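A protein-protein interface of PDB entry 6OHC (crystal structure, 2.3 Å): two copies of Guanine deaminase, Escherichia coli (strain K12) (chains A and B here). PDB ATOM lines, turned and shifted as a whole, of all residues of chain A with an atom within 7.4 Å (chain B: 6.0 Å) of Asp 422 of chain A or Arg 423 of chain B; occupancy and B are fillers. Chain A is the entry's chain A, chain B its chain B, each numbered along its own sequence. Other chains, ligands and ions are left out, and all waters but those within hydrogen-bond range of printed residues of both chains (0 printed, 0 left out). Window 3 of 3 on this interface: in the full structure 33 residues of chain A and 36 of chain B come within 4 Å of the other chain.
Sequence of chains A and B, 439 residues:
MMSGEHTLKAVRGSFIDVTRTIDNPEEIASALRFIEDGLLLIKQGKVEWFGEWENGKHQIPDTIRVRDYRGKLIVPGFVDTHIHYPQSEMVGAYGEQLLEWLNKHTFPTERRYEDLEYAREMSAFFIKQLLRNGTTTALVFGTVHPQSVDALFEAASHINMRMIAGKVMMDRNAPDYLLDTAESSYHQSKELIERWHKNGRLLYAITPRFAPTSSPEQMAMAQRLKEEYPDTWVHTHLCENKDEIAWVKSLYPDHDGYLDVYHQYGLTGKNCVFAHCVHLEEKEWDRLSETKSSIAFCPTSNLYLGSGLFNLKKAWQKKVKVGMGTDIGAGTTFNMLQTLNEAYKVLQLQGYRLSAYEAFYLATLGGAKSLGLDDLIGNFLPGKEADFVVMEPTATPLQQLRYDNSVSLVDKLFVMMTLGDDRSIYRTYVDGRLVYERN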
ATOM      1  N   GLN A 129      23.625  -1.690  32.719  1.00  0.00           N
ATOM      2  CA  GLN A 129      23.280  -0.667  31.694  1.00  0.00           C
ATOM      3  C   GLN A 129      23.772   0.706  32.116  1.00  0.00           C
ATOM      4  O   GLN A 129      24.322   1.409  31.242  1.00  0.00           O
ATOM      5  CB  GLN A 129      21.784  -0.605  31.385  1.00  0.00           C
ATOM      6  CG  GLN A 129      21.335  -1.853  30.631  1.00  0.00           C
ATOM      7  CD  GLN A 129      21.992  -1.937  29.271  1.00  0.00           C
ATOM      8  OE1 GLN A 129      21.764  -1.095  28.399  1.00  0.00           O
ATOM      9  NE2 GLN A 129      22.862  -2.920  29.086  1.00  0.00           N
ATOM     10  N   LEU A 131      26.390   1.296  34.247  1.00  0.00           N
ATOM     11  CA  LEU A 131      27.900   1.282  34.279  1.00  0.00           C
ATOM     12  C   LEU A 131      28.436   1.296  32.822  1.00  0.00           C
ATOM     13  O   LEU A 131      29.385   2.029  32.489  1.00  0.00           O
ATOM     14  CB  LEU A 131      28.393   0.033  35.011  1.00  0.00           C
ATOM     15  CG  LEU A 131      27.964  -0.141  36.468  1.00  0.00           C
ATOM     16  CD1 LEU A 131      28.588  -1.386  37.063  1.00  0.00           C
ATOM     17  CD2 LEU A 131      28.354   1.085  37.280  1.00  0.00           C
ATOM     18  N   ARG A 132      27.845   0.474  31.967  1.00  0.00           N
ATOM     19  CA  ARG A 132      28.201   0.392  30.541  1.00  0.00           C
ATOM     20  C   ARG A 132      28.058   1.786  29.881  1.00  0.00           C
ATOM     21  O   ARG A 132      28.706   2.013  28.881  1.00  0.00           O
ATOM     22  CB  ARG A 132      27.310  -0.673  29.911  1.00  0.00           C
ATOM     23  CG  ARG A 132      27.336  -0.640  28.396  1.00  0.00           C
ATOM     24  CD  ARG A 132      26.103  -1.151  27.695  1.00  0.00           C
ATOM     25  NE  ARG A 132      26.165  -2.585  27.764  1.00  0.00           N
ATOM     26  CZ  ARG A 132      26.776  -3.351  26.863  1.00  0.00           C
ATOM     27  NH1 ARG A 132      27.398  -2.807  25.823  1.00  0.00           N
ATOM     28  NH2 ARG A 132      26.737  -4.660  27.016  1.00  0.00           N
ATOM     29  N   ASN A 133      27.228   2.672  30.444  1.00  0.00           N
ATOM     30  CA  ASN A 133      26.946   4.034  29.932  1.00  0.00           C
ATOM     31  C   ASN A 133      27.636   5.114  30.764  1.00  0.00           C
ATOM     32  O   ASN A 133      27.453   6.254  30.454  1.00  0.00           O
ATOM     33  CB  ASN A 133      25.455   4.276  29.749  1.00  0.00           C
ATOM     34  CG  ASN A 133      24.974   3.624  28.471  1.00  0.00           C
ATOM     35  OD1 ASN A 133      25.264   4.116  27.353  1.00  0.00           O
ATOM     36  ND2 ASN A 133      24.374   2.451  28.608  1.00  0.00           N
ATOM     37  N   GLY A 134      28.463   4.764  31.717  1.00  0.00           N
ATOM     38  CA  GLY A 134      29.214   5.727  32.547  1.00  0.00           C
ATOM     39  C   GLY A 134      28.346   6.419  33.604  1.00  0.00           C
ATOM     40  O   GLY A 134      28.793   7.425  34.176  1.00  0.00           O
ATOM     41  N   THR A 333      17.249   5.627  25.739  1.00  0.00           N
ATOM     42  CA  THR A 333      18.700   5.453  25.997  1.00  0.00           C
ATOM     43  C   THR A 333      19.029   5.695  27.481  1.00  0.00           C
ATOM     44  O   THR A 333      18.494   6.615  28.077  1.00  0.00           O
ATOM     45  CB  THR A 333      19.530   6.369  25.098  1.00  0.00           C
ATOM     46  OG1 THR A 333      20.897   6.064  25.373  1.00  0.00           O
ATOM     47  CG2 THR A 333      19.303   7.856  25.346  1.00  0.00           C
ATOM     48  N   PHE A 334      19.969   4.885  27.974  1.00  0.00           N
ATOM     49  CA  PHE A 334      20.657   4.992  29.286  1.00  0.00           C
ATOM     50  C   PHE A 334      21.784   6.017  29.215  1.00  0.00           C
ATOM     51  O   PHE A 334      22.309   6.436  30.286  1.00  0.00           O
ATOM     52  CB  PHE A 334      21.231   3.617  29.650  1.00  0.00           C
ATOM     53  CG  PHE A 334      20.200   2.639  30.161  1.00  0.00           C
ATOM     54  CD1 PHE A 334      19.408   1.947  29.268  1.00  0.00           C
ATOM     55  CD2 PHE A 334      20.027   2.427  31.523  1.00  0.00           C
ATOM     56  CE1 PHE A 334      18.479   1.025  29.723  1.00  0.00           C
ATOM     57  CE2 PHE A 334      19.047   1.561  31.968  1.00  0.00           C
ATOM     58  CZ  PHE A 334      18.294   0.833  31.066  1.00  0.00           C
ATOM     59  N   ASN A 335      22.177   6.382  27.990  1.00  0.00           N
ATOM     60  CA  ASN A 335      23.437   7.121  27.765  1.00  0.00           C
ATOM     61  C   ASN A 335      23.244   8.619  28.060  1.00  0.00           C
ATOM     62  O   ASN A 335      22.374   9.288  27.448  1.00  0.00           O
ATOM     63  CB  ASN A 335      23.957   6.889  26.357  1.00  0.00           C
ATOM     64  CG  ASN A 335      25.407   7.313  26.264  1.00  0.00           C
ATOM     65  OD1 ASN A 335      25.676   8.447  25.885  1.00  0.00           O
ATOM     66  ND2 ASN A 335      26.338   6.453  26.669  1.00  0.00           N
ATOM     67  N   LEU A 337      25.481  10.966  27.306  1.00  0.00           N
ATOM     68  CA  LEU A 337      25.970  11.769  26.133  1.00  0.00           C
ATOM     69  C   LEU A 337      24.817  11.950  25.127  1.00  0.00           C
ATOM     70  O   LEU A 337      24.598  13.081  24.728  1.00  0.00           O
ATOM     71  CB  LEU A 337      27.137  11.067  25.470  1.00  0.00           C
ATOM     72  CG  LEU A 337      28.315  10.748  26.345  1.00  0.00           C
ATOM     73  CD1 LEU A 337      29.271   9.833  25.541  1.00  0.00           C
ATOM     74  CD2 LEU A 337      28.995  12.014  26.783  1.00  0.00           C
ATOM     75  N   GLN A 338      24.076  10.861  24.804  1.00  0.00           N
ATOM     76  CA  GLN A 338      22.890  10.936  23.925  1.00  0.00           C
ATOM     77  C   GLN A 338      21.830  11.831  24.558  1.00  0.00           C
ATOM     78  O   GLN A 338      21.197  12.564  23.829  1.00  0.00           O
ATOM     79  CB  GLN A 338      22.357   9.543  23.624  1.00  0.00           C
ATOM     80  CG  GLN A 338      23.357   8.736  22.806  1.00  0.00           C
ATOM     81  CD  GLN A 338      22.751   7.457  22.297  1.00  0.00           C
ATOM     82  OE1 GLN A 338      21.999   6.799  23.029  1.00  0.00           O
ATOM     83  NE2 GLN A 338      23.029   7.115  21.059  1.00  0.00           N
ATOM     84  N   GLU A 392      36.428   7.401  25.333  1.00  0.00           N
ATOM     85  CA  GLU A 392      37.171   7.599  24.067  1.00  0.00           C
ATOM     86  C   GLU A 392      36.192   7.784  22.933  1.00  0.00           C
ATOM     87  O   GLU A 392      35.086   7.281  22.976  1.00  0.00           O
ATOM     88  CB  GLU A 392      38.116   6.449  23.769  1.00  0.00           C
ATOM     89  CG  GLU A 392      37.463   5.124  23.867  1.00  0.00           C
ATOM     90  CD  GLU A 392      38.323   3.972  23.386  1.00  0.00           C
ATOM     91  OE1 GLU A 392      38.243   2.897  24.018  1.00  0.00           O
ATOM     92  OE2 GLU A 392      39.040   4.115  22.371  1.00  0.00           O
ATOM     93  N   ALA A 395      33.147   5.313  19.044  1.00  0.00           N
ATOM     94  CA  ALA A 395      31.774   4.772  18.926  1.00  0.00           C
ATOM     95  C   ALA A 395      31.493   4.439  17.462  1.00  0.00           C
ATOM     96  O   ALA A 395      30.854   3.412  17.225  1.00  0.00           O
ATOM     97  CB  ALA A 395      30.743   5.767  19.443  1.00  0.00           C
ATOM     98  N   LEU A 419      28.057  12.614  18.953  1.00  0.00           N
ATOM     99  CA  LEU A 419      28.265  11.292  18.316  1.00  0.00           C
ATOM    100  C   LEU A 419      28.620  10.209  19.340  1.00  0.00           C
ATOM    101  O   LEU A 419      28.978   9.127  18.942  1.00  0.00           O
ATOM    102  CB  LEU A 419      29.388  11.411  17.297  1.00  0.00           C
ATOM    103  CG  LEU A 419      29.015  12.068  15.968  1.00  0.00           C
ATOM    104  CD1 LEU A 419      29.101  13.583  16.071  1.00  0.00           C
ATOM    105  CD2 LEU A 419      29.957  11.544  14.899  1.00  0.00           C
ATOM    106  N   GLY A 420      28.525  10.479  20.632  1.00  0.00           N
ATOM    107  CA  GLY A 420      28.779   9.478  21.685  1.00  0.00           C
ATOM    108  C   GLY A 420      27.601   8.539  21.877  1.00  0.00           C
ATOM    109  O   GLY A 420      26.457   8.964  21.622  1.00  0.00           O
ATOM    110  N   ASP A 421      27.901   7.279  22.184  1.00  0.00           N
ATOM    111  CA  ASP A 421      26.939   6.280  22.697  1.00  0.00           C
ATOM    112  C   ASP A 421      27.723   5.451  23.710  1.00  0.00           C
ATOM    113  O   ASP A 421      28.776   5.897  24.148  1.00  0.00           O
ATOM    114  CB  ASP A 421      26.262   5.511  21.548  1.00  0.00           C
ATOM    115  CG  ASP A 421      27.169   4.623  20.719  1.00  0.00           C
ATOM    116  OD1 ASP A 421      28.079   3.993  21.288  1.00  0.00           O
ATOM    117  OD2 ASP A 421      26.970   4.547  19.514  1.00  0.00           O
ATOM    118  N   ASP A 422      27.221   4.286  24.068  1.00  0.00           N
ATOM    119  CA  ASP A 422      27.842   3.367  25.063  1.00  0.00           C
ATOM    120  C   ASP A 422      29.250   2.964  24.634  1.00  0.00           C
ATOM    121  O   ASP A 422      30.076   2.754  25.509  1.00  0.00           O
ATOM    122  CB  ASP A 422      26.940   2.150  25.330  1.00  0.00           C
ATOM    123  CG  ASP A 422      26.587   1.397  24.082  1.00  0.00           C
ATOM    124  OD1 ASP A 422      25.721   1.878  23.298  1.00  0.00           O
ATOM    125  OD2 ASP A 422      27.179   0.369  23.886  1.00  0.00           O
ATOM    126  N   ARG A 423      29.542   2.912  23.338  1.00  0.00           N
ATOM    127  CA  ARG A 423      30.873   2.450  22.881  1.00  0.00           C
ATOM    128  C   ARG A 423      31.951   3.463  23.274  1.00  0.00           C
ATOM    129  O   ARG A 423      33.131   3.071  23.339  1.00  0.00           O
ATOM    130  CB  ARG A 423      30.850   2.153  21.385  1.00  0.00           C
ATOM    131  CG  ARG A 423      30.010   0.909  21.080  1.00  0.00           C
ATOM    132  CD  ARG A 423      29.760   0.793  19.593  1.00  0.00           C
ATOM    133  NE  ARG A 423      28.841   1.827  19.082  1.00  0.00           N
ATOM    134  CZ  ARG A 423      28.462   1.905  17.830  1.00  0.00           C
ATOM    135  NH1 ARG A 423      28.883   1.011  16.943  1.00  0.00           N
ATOM    136  NH2 ARG A 423      27.656   2.883  17.474  1.00  0.00           N
ATOM    137  N   SER A 424      31.579   4.703  23.546  1.00  0.00           N
ATOM    138  CA  SER A 424      32.520   5.758  24.014  1.00  0.00           C
ATOM    139  C   SER A 424      32.999   5.471  25.448  1.00  0.00           C
ATOM    140  O   SER A 424      33.998   6.047  25.814  1.00  0.00           O
ATOM    141  CB  SER A 424      31.854   7.109  23.964  1.00  0.00           C
ATOM    142  OG  SER A 424      31.522   7.474  22.655  1.00  0.00           O
ATOM    143  N   ILE A 425      32.282   4.645  26.227  1.00  0.00           N
ATOM    144  CA  ILE A 425      32.647   4.336  27.624  1.00  0.00           C
ATOM    145  C   ILE A 425      33.583   3.127  27.612  1.00  0.00           C
ATOM    146  O   ILE A 425      33.125   2.031  27.282  1.00  0.00           O
ATOM    147  CB  ILE A 425      31.392   4.121  28.518  1.00  0.00           C
ATOM    148  CG1 ILE A 425      30.585   5.401  28.789  1.00  0.00           C
ATOM    149  CG2 ILE A 425      31.800   3.502  29.852  1.00  0.00           C
ATOM    150  CD1 ILE A 425      30.369   6.288  27.622  1.00  0.00           C
ATOM    151  N   TYR A 426      34.865   3.338  27.922  1.00  0.00           N
ATOM    152  CA  TYR A 426      35.936   2.318  27.968  1.00  0.00           C
ATOM    153  C   TYR A 426      35.979   1.646  29.342  1.00  0.00           C
ATOM    154  O   TYR A 426      36.226   0.430  29.390  1.00  0.00           O
ATOM    155  CB  TYR A 426      37.264   3.006  27.672  1.00  0.00           C
ATOM    156  CG  TYR A 426      38.492   2.140  27.666  1.00  0.00           C
ATOM    157  CD1 TYR A 426      38.692   1.197  26.670  1.00  0.00           C
ATOM    158  CD2 TYR A 426      39.484   2.292  28.609  1.00  0.00           C
ATOM    159  CE1 TYR A 426      39.828   0.406  26.625  1.00  0.00           C
ATOM    160  CE2 TYR A 426      40.602   1.473  28.615  1.00  0.00           C
ATOM    161  CZ  TYR A 426      40.792   0.540  27.611  1.00  0.00           C
ATOM    162  OH  TYR A 426      41.958  -0.184  27.577  1.00  0.00           O
ATOM    163  N   TYR A 436      33.458  -1.971  35.533  1.00  0.00           N
ATOM    164  CA  TYR A 436      33.023  -2.179  34.143  1.00  0.00           C
ATOM    165  C   TYR A 436      34.192  -1.872  33.203  1.00  0.00           C
ATOM    166  O   TYR A 436      34.776  -0.775  33.332  1.00  0.00           O
ATOM    167  CB  TYR A 436      31.808  -1.323  33.779  1.00  0.00           C
ATOM    168  CG  TYR A 436      31.481  -1.400  32.310  1.00  0.00           C
ATOM    169  CD1 TYR A 436      30.781  -2.476  31.802  1.00  0.00           C
ATOM    170  CD2 TYR A 436      31.968  -0.451  31.417  1.00  0.00           C
ATOM    171  CE1 TYR A 436      30.499  -2.586  30.444  1.00  0.00           C
ATOM    172  CE2 TYR A 436      31.721  -0.547  30.056  1.00  0.00           C
ATOM    173  CZ  TYR A 436      30.999  -1.637  29.570  1.00  0.00           C
ATOM    174  OH  TYR A 436      30.757  -1.765  28.254  1.00  0.00           O
ATOM    175  N   ARG A 438      34.596  -2.205  28.802  1.00  0.00           N
ATOM    176  CA  ARG A 438      34.065  -2.551  27.466  1.00  0.00           C
ATOM    177  C   ARG A 438      34.846  -3.770  26.934  1.00  0.00           C
ATOM    178  O   ARG A 438      36.086  -3.772  26.988  1.00  0.00           O
ATOM    179  CB  ARG A 438      34.206  -1.328  26.559  1.00  0.00           C
ATOM    180  CG  ARG A 438      33.289  -1.366  25.343  1.00  0.00           C
ATOM    181  CD  ARG A 438      33.550  -0.313  24.297  1.00  0.00           C
ATOM    182  NE  ARG A 438      34.954  -0.342  23.953  1.00  0.00           N
ATOM    183  CZ  ARG A 438      35.784   0.699  23.855  1.00  0.00           C
ATOM    184  NH1 ARG A 438      35.371   1.938  24.061  1.00  0.00           N
ATOM    185  NH2 ARG A 438      37.060   0.471  23.592  1.00  0.00           N
ATOM    186  N   ARG B 132      28.465   0.167   5.818  1.00  0.00           N
ATOM    187  CA  ARG B 132      28.518  -0.183   7.249  1.00  0.00           C
ATOM    188  C   ARG B 132      27.180   0.135   7.917  1.00  0.00           C
ATOM    189  O   ARG B 132      26.875  -0.504   8.938  1.00  0.00           O
ATOM    190  CB  ARG B 132      29.713   0.565   7.839  1.00  0.00           C
ATOM    191  CG  ARG B 132      29.760   0.581   9.348  1.00  0.00           C
ATOM    192  CD  ARG B 132      30.895   1.471   9.776  1.00  0.00           C
ATOM    193  NE  ARG B 132      30.945   1.142  11.186  1.00  0.00           N
ATOM    194  CZ  ARG B 132      31.928   0.489  11.748  1.00  0.00           C
ATOM    195  NH1 ARG B 132      32.999   0.140  11.063  1.00  0.00           N
ATOM    196  NH2 ARG B 132      31.889   0.283  13.045  1.00  0.00           N
ATOM    197  N   ASN B 335      23.409   6.565   9.696  1.00  0.00           N
ATOM    198  CA  ASN B 335      22.504   5.437   9.992  1.00  0.00           C
ATOM    199  C   ASN B 335      21.050   5.828   9.726  1.00  0.00           C
ATOM    200  O   ASN B 335      20.511   6.820  10.342  1.00  0.00           O
ATOM    201  CB  ASN B 335      22.672   4.953  11.423  1.00  0.00           C
ATOM    202  CG  ASN B 335      22.063   3.583  11.598  1.00  0.00           C
ATOM    203  OD1 ASN B 335      20.893   3.490  11.958  1.00  0.00           O
ATOM    204  ND2 ASN B 335      22.808   2.549  11.236  1.00  0.00           N
ATOM    205  N   GLU B 392      20.930  -7.832  12.262  1.00  0.00           N
ATOM    206  CA  GLU B 392      20.829  -8.485  13.571  1.00  0.00           C
ATOM    207  C   GLU B 392      20.199  -7.467  14.498  1.00  0.00           C
ATOM    208  O   GLU B 392      20.895  -6.697  15.133  1.00  0.00           O
ATOM    209  CB  GLU B 392      22.228  -8.848  14.070  1.00  0.00           C
ATOM    210  CG  GLU B 392      22.242  -9.611  15.398  1.00  0.00           C
ATOM    211  CD  GLU B 392      23.668  -9.866  15.806  1.00  0.00           C
ATOM    212  OE1 GLU B 392      24.541  -9.335  15.133  1.00  0.00           O
ATOM    213  OE2 GLU B 392      23.881 -10.530  16.844  1.00  0.00           O
ATOM    214  N   ALA B 395      21.597  -7.198  18.217  1.00  0.00           N
ATOM    215  CA  ALA B 395      23.059  -6.952  18.207  1.00  0.00           C
ATOM    216  C   ALA B 395      23.557  -6.478  19.584  1.00  0.00           C
ATOM    217  O   ALA B 395      24.610  -6.947  19.952  1.00  0.00           O
ATOM    218  CB  ALA B 395      23.437  -5.995  17.099  1.00  0.00           C
ATOM    219  N   THR B 396      22.797  -5.699  20.367  1.00  0.00           N
ATOM    220  CA  THR B 396      23.174  -5.299  21.768  1.00  0.00           C
ATOM    221  C   THR B 396      22.253  -5.977  22.773  1.00  0.00           C
ATOM    222  O   THR B 396      21.197  -6.462  22.425  1.00  0.00           O
ATOM    223  CB  THR B 396      23.195  -3.773  21.926  1.00  0.00           C
ATOM    224  OG1 THR B 396      21.885  -3.207  21.816  1.00  0.00           O
ATOM    225  CG2 THR B 396      24.043  -3.088  20.856  1.00  0.00           C
ATOM    226  N   ASP B 421      21.251   0.814  15.680  1.00  0.00           N
ATOM    227  CA  ASP B 421      22.345   1.646  15.136  1.00  0.00           C
ATOM    228  C   ASP B 421      23.142   0.794  14.149  1.00  0.00           C
ATOM    229  O   ASP B 421      22.588  -0.165  13.678  1.00  0.00           O
ATOM    230  CB  ASP B 421      23.128   2.294  16.277  1.00  0.00           C
ATOM    231  CG  ASP B 421      23.909   1.338  17.158  1.00  0.00           C
ATOM    232  OD1 ASP B 421      24.435   0.336  16.640  1.00  0.00           O
ATOM    233  OD2 ASP B 421      24.044   1.647  18.348  1.00  0.00           O
ATOM    234  N   ASP B 422      24.394   1.147  13.860  1.00  0.00           N
ATOM    235  CA  ASP B 422      25.257   0.464  12.871  1.00  0.00           C
ATOM    236  C   ASP B 422      25.499  -0.974  13.346  1.00  0.00           C
ATOM    237  O   ASP B 422      25.759  -1.857  12.454  1.00  0.00           O
ATOM    238  CB  ASP B 422      26.562   1.215  12.628  1.00  0.00           C
ATOM    239  CG  ASP B 422      27.312   1.487  13.919  1.00  0.00           C
ATOM    240  OD1 ASP B 422      26.905   2.377  14.666  1.00  0.00           O
ATOM    241  OD2 ASP B 422      28.298   0.788  14.181  1.00  0.00           O
ATOM    242  N   ARG B 423      25.423  -1.259  14.651  1.00  0.00           N
ATOM    243  CA  ARG B 423      25.693  -2.635  15.122  1.00  0.00           C
ATOM    244  C   ARG B 423      24.631  -3.616  14.579  1.00  0.00           C
ATOM    245  O   ARG B 423      24.910  -4.838  14.552  1.00  0.00           O
ATOM    246  CB  ARG B 423      25.803  -2.691  16.646  1.00  0.00           C
ATOM    247  CG  ARG B 423      27.116  -2.093  17.116  1.00  0.00           C
ATOM    248  CD  ARG B 423      27.155  -1.828  18.602  1.00  0.00           C
ATOM    249  NE  ARG B 423      26.259  -0.753  18.989  1.00  0.00           N
ATOM    250  CZ  ARG B 423      26.193  -0.255  20.231  1.00  0.00           C
ATOM    251  NH1 ARG B 423      26.963  -0.737  21.188  1.00  0.00           N
ATOM    252  NH2 ARG B 423      25.325   0.694  20.512  1.00  0.00           N
ATOM    253  N   SER B 424      23.481  -3.119  14.167  1.00  0.00           N
ATOM    254  CA  SER B 424      22.378  -3.917  13.614  1.00  0.00           C
ATOM    255  C   SER B 424      22.755  -4.411  12.204  1.00  0.00           C
ATOM    256  O   SER B 424      22.100  -5.308  11.736  1.00  0.00           O
ATOM    257  CB  SER B 424      21.118  -3.069  13.547  1.00  0.00           C
ATOM    258  OG  SER B 424      20.677  -2.733  14.842  1.00  0.00           O
ATOM    259  N   ILE B 425      23.702  -3.766  11.520  1.00  0.00           N
ATOM    260  CA  ILE B 425      24.035  -4.097  10.099  1.00  0.00           C
ATOM    261  C   ILE B 425      25.142  -5.158  10.121  1.00  0.00           C
ATOM    262  O   ILE B 425      26.299  -4.816  10.488  1.00  0.00           O
ATOM    263  CB  ILE B 425      24.415  -2.856   9.269  1.00  0.00           C
ATOM    264  CG1 ILE B 425      23.195  -1.956   8.991  1.00  0.00           C
ATOM    265  CG2 ILE B 425      24.980  -3.309   7.932  1.00  0.00           C
ATOM    266  CD1 ILE B 425      22.365  -1.609  10.179  1.00  0.00           C
ATOM    267  N   TYR B 426      24.783  -6.405   9.792  1.00  0.00           N
ATOM    268  CA  TYR B 426      25.685  -7.570   9.840  1.00  0.00           C
ATOM    269  C   TYR B 426      26.371  -7.749   8.498  1.00  0.00           C
ATOM    270  O   TYR B 426      27.564  -8.117   8.476  1.00  0.00           O
ATOM    271  CB  TYR B 426      24.859  -8.796  10.155  1.00  0.00           C
ATOM    272  CG  TYR B 426      25.612 -10.071  10.325  1.00  0.00           C
ATOM    273  CD1 TYR B 426      26.445 -10.254  11.421  1.00  0.00           C
ATOM    274  CD2 TYR B 426      25.399 -11.137   9.473  1.00  0.00           C
ATOM    275  CE1 TYR B 426      27.111 -11.456  11.621  1.00  0.00           C
ATOM    276  CE2 TYR B 426      26.028 -12.346   9.678  1.00  0.00           C
ATOM    277  CZ  TYR B 426      26.888 -12.507  10.748  1.00  0.00           C
ATOM    278  OH  TYR B 426      27.535 -13.693  10.977  1.00  0.00           O
ATOM    279  N   ARG B 438      30.351  -6.865   9.151  1.00  0.00           N
ATOM    280  CA  ARG B 438      30.688  -6.345  10.508  1.00  0.00           C
ATOM    281  C   ARG B 438      31.913  -7.096  11.047  1.00  0.00           C
ATOM    282  O   ARG B 438      31.891  -8.351  11.005  1.00  0.00           O
ATOM    283  CB  ARG B 438      29.450  -6.413  11.403  1.00  0.00           C
ATOM    284  CG  ARG B 438      29.549  -5.487  12.606  1.00  0.00           C
ATOM    285  CD  ARG B 438      28.311  -5.245  13.442  1.00  0.00           C
ATOM    286  NE  ARG B 438      27.882  -6.298  14.354  1.00  0.00           N
ATOM    287  CZ  ARG B 438      27.999  -6.262  15.700  1.00  0.00           C
ATOM    288  NH1 ARG B 438      28.624  -5.268  16.320  1.00  0.00           N
ATOM    289  NH2 ARG B 438      27.522  -7.265  16.420  1.00  0.00           N
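Among the printed residues, merely in contact across the chains: Arg 423 of chain A with Arg 423 of chain B (3.5 Å).
Printed residues of chain A that touch a printed residue of chain B: Asp 422 and Arg 423. Among the printed residues, 4 pairs touch across the chains. Among the printed residues, Asp or Glu carboxylates within 4 Å of a Lys or Arg side-chain nitrogen of the other chain: Asp 422 of chain A with Arg 423 of chain B, Arg 423 of chain A with Asp 421 of chain B and Arg 423 of chain A with Asp 422 of chain B.
Asp 422 of chain A touches Arg 423 of chain B, and with the chains exchanged Arg 423 of chain A touches Asp 422 of chain B. Arg 423 of chain A touches Asp 421 of chain B, but with the chains exchanged Asp 421 of chain A does not touch Arg 423 of chain B (4.3 Å). Arg 423 of chain B touches its own counterpart, Arg 423 of chain A. 11 positions are printed for both chains. Of the 4 pairs that touch across the chains among the printed residues, 3 have their exchanged pair printed and touching as well.
NH1 of Arg 423 of chain B is in salt-bridge range of OD2 of Asp 422 of chain A, at 2.9 Å. The guanidinium group of Arg 423 of chain A lies within salt-bridge range of the side-chain carboxylate of Asp 422 of chain B, 2.8 Å away. The guanidinium group (NH2) of Arg 423 of chain A lies within salt-bridge range of the side-chain carboxylate (OD2) of Asp 421 of chain B (3.9 Å).
The side-chain carboxylate (OD2) of Asp 422 of chain B is in salt-bridge range of the guanidinium group (NH2) of Arg 132 of chain B, at 3.8 Å. The backbone carbonyl oxygen (O) of Ala 395 of chain A sits close to the guanidinium group (NH1) of Arg 423 of chain A, 3.1 Å away. The guanidinium group (NH1) of Arg 438 of chain A is in hydrogen-bond range of the backbone carbonyl oxygen (O) of Arg 423 of chain A, at 2.6 Å. The side-chain carboxylate (OD2) of Asp 422 of chain A lies within salt-bridge range of the guanidinium group (NH1) of Arg 132 of chain A. The side-chain amide nitrogen (ND2) of Asn 335 of chain A lies close to the backbone NH (N) of Asp 422 of chain A, 3.5 Å away. The side-chain amide nitrogen (ND2) of Asn 335 of chain B lies close to the backbone NH (N) of Asp 422 of chain B (3.4 Å).
Asp 422 of chain A touches just one residue of chain B: Arg 423 (2.9 Å). Of the printed residues of chain A, Arg 423 of chain B touches Asp 422 and Arg 423. Of the printed residues of chain A, Asp 422 of chain B touches Arg 423. Printed residues of chain B within 4 Å of Arg 423 of chain A: Asp 421 (3.9 Å), Asp 422 (2.8 Å) and Arg 423 (3.5 Å). Of the printed residues of chain A, Asp 421 of chain B touches Arg 423. Ser 424 of chain B touches none of the printed residues of chain A. The nearest residue of chain B that does not touch Asp 422 of chain A is Asp 421 of chain B (5.2 Å). The nearest residue of chain A that does not touch Arg 423 of chain B is Asp 421 of chain A (4.3 Å). The nearest printed residue of chain A that does not touch Asp 422 of chain B is Ala 395 of chain A (4.8 Å).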
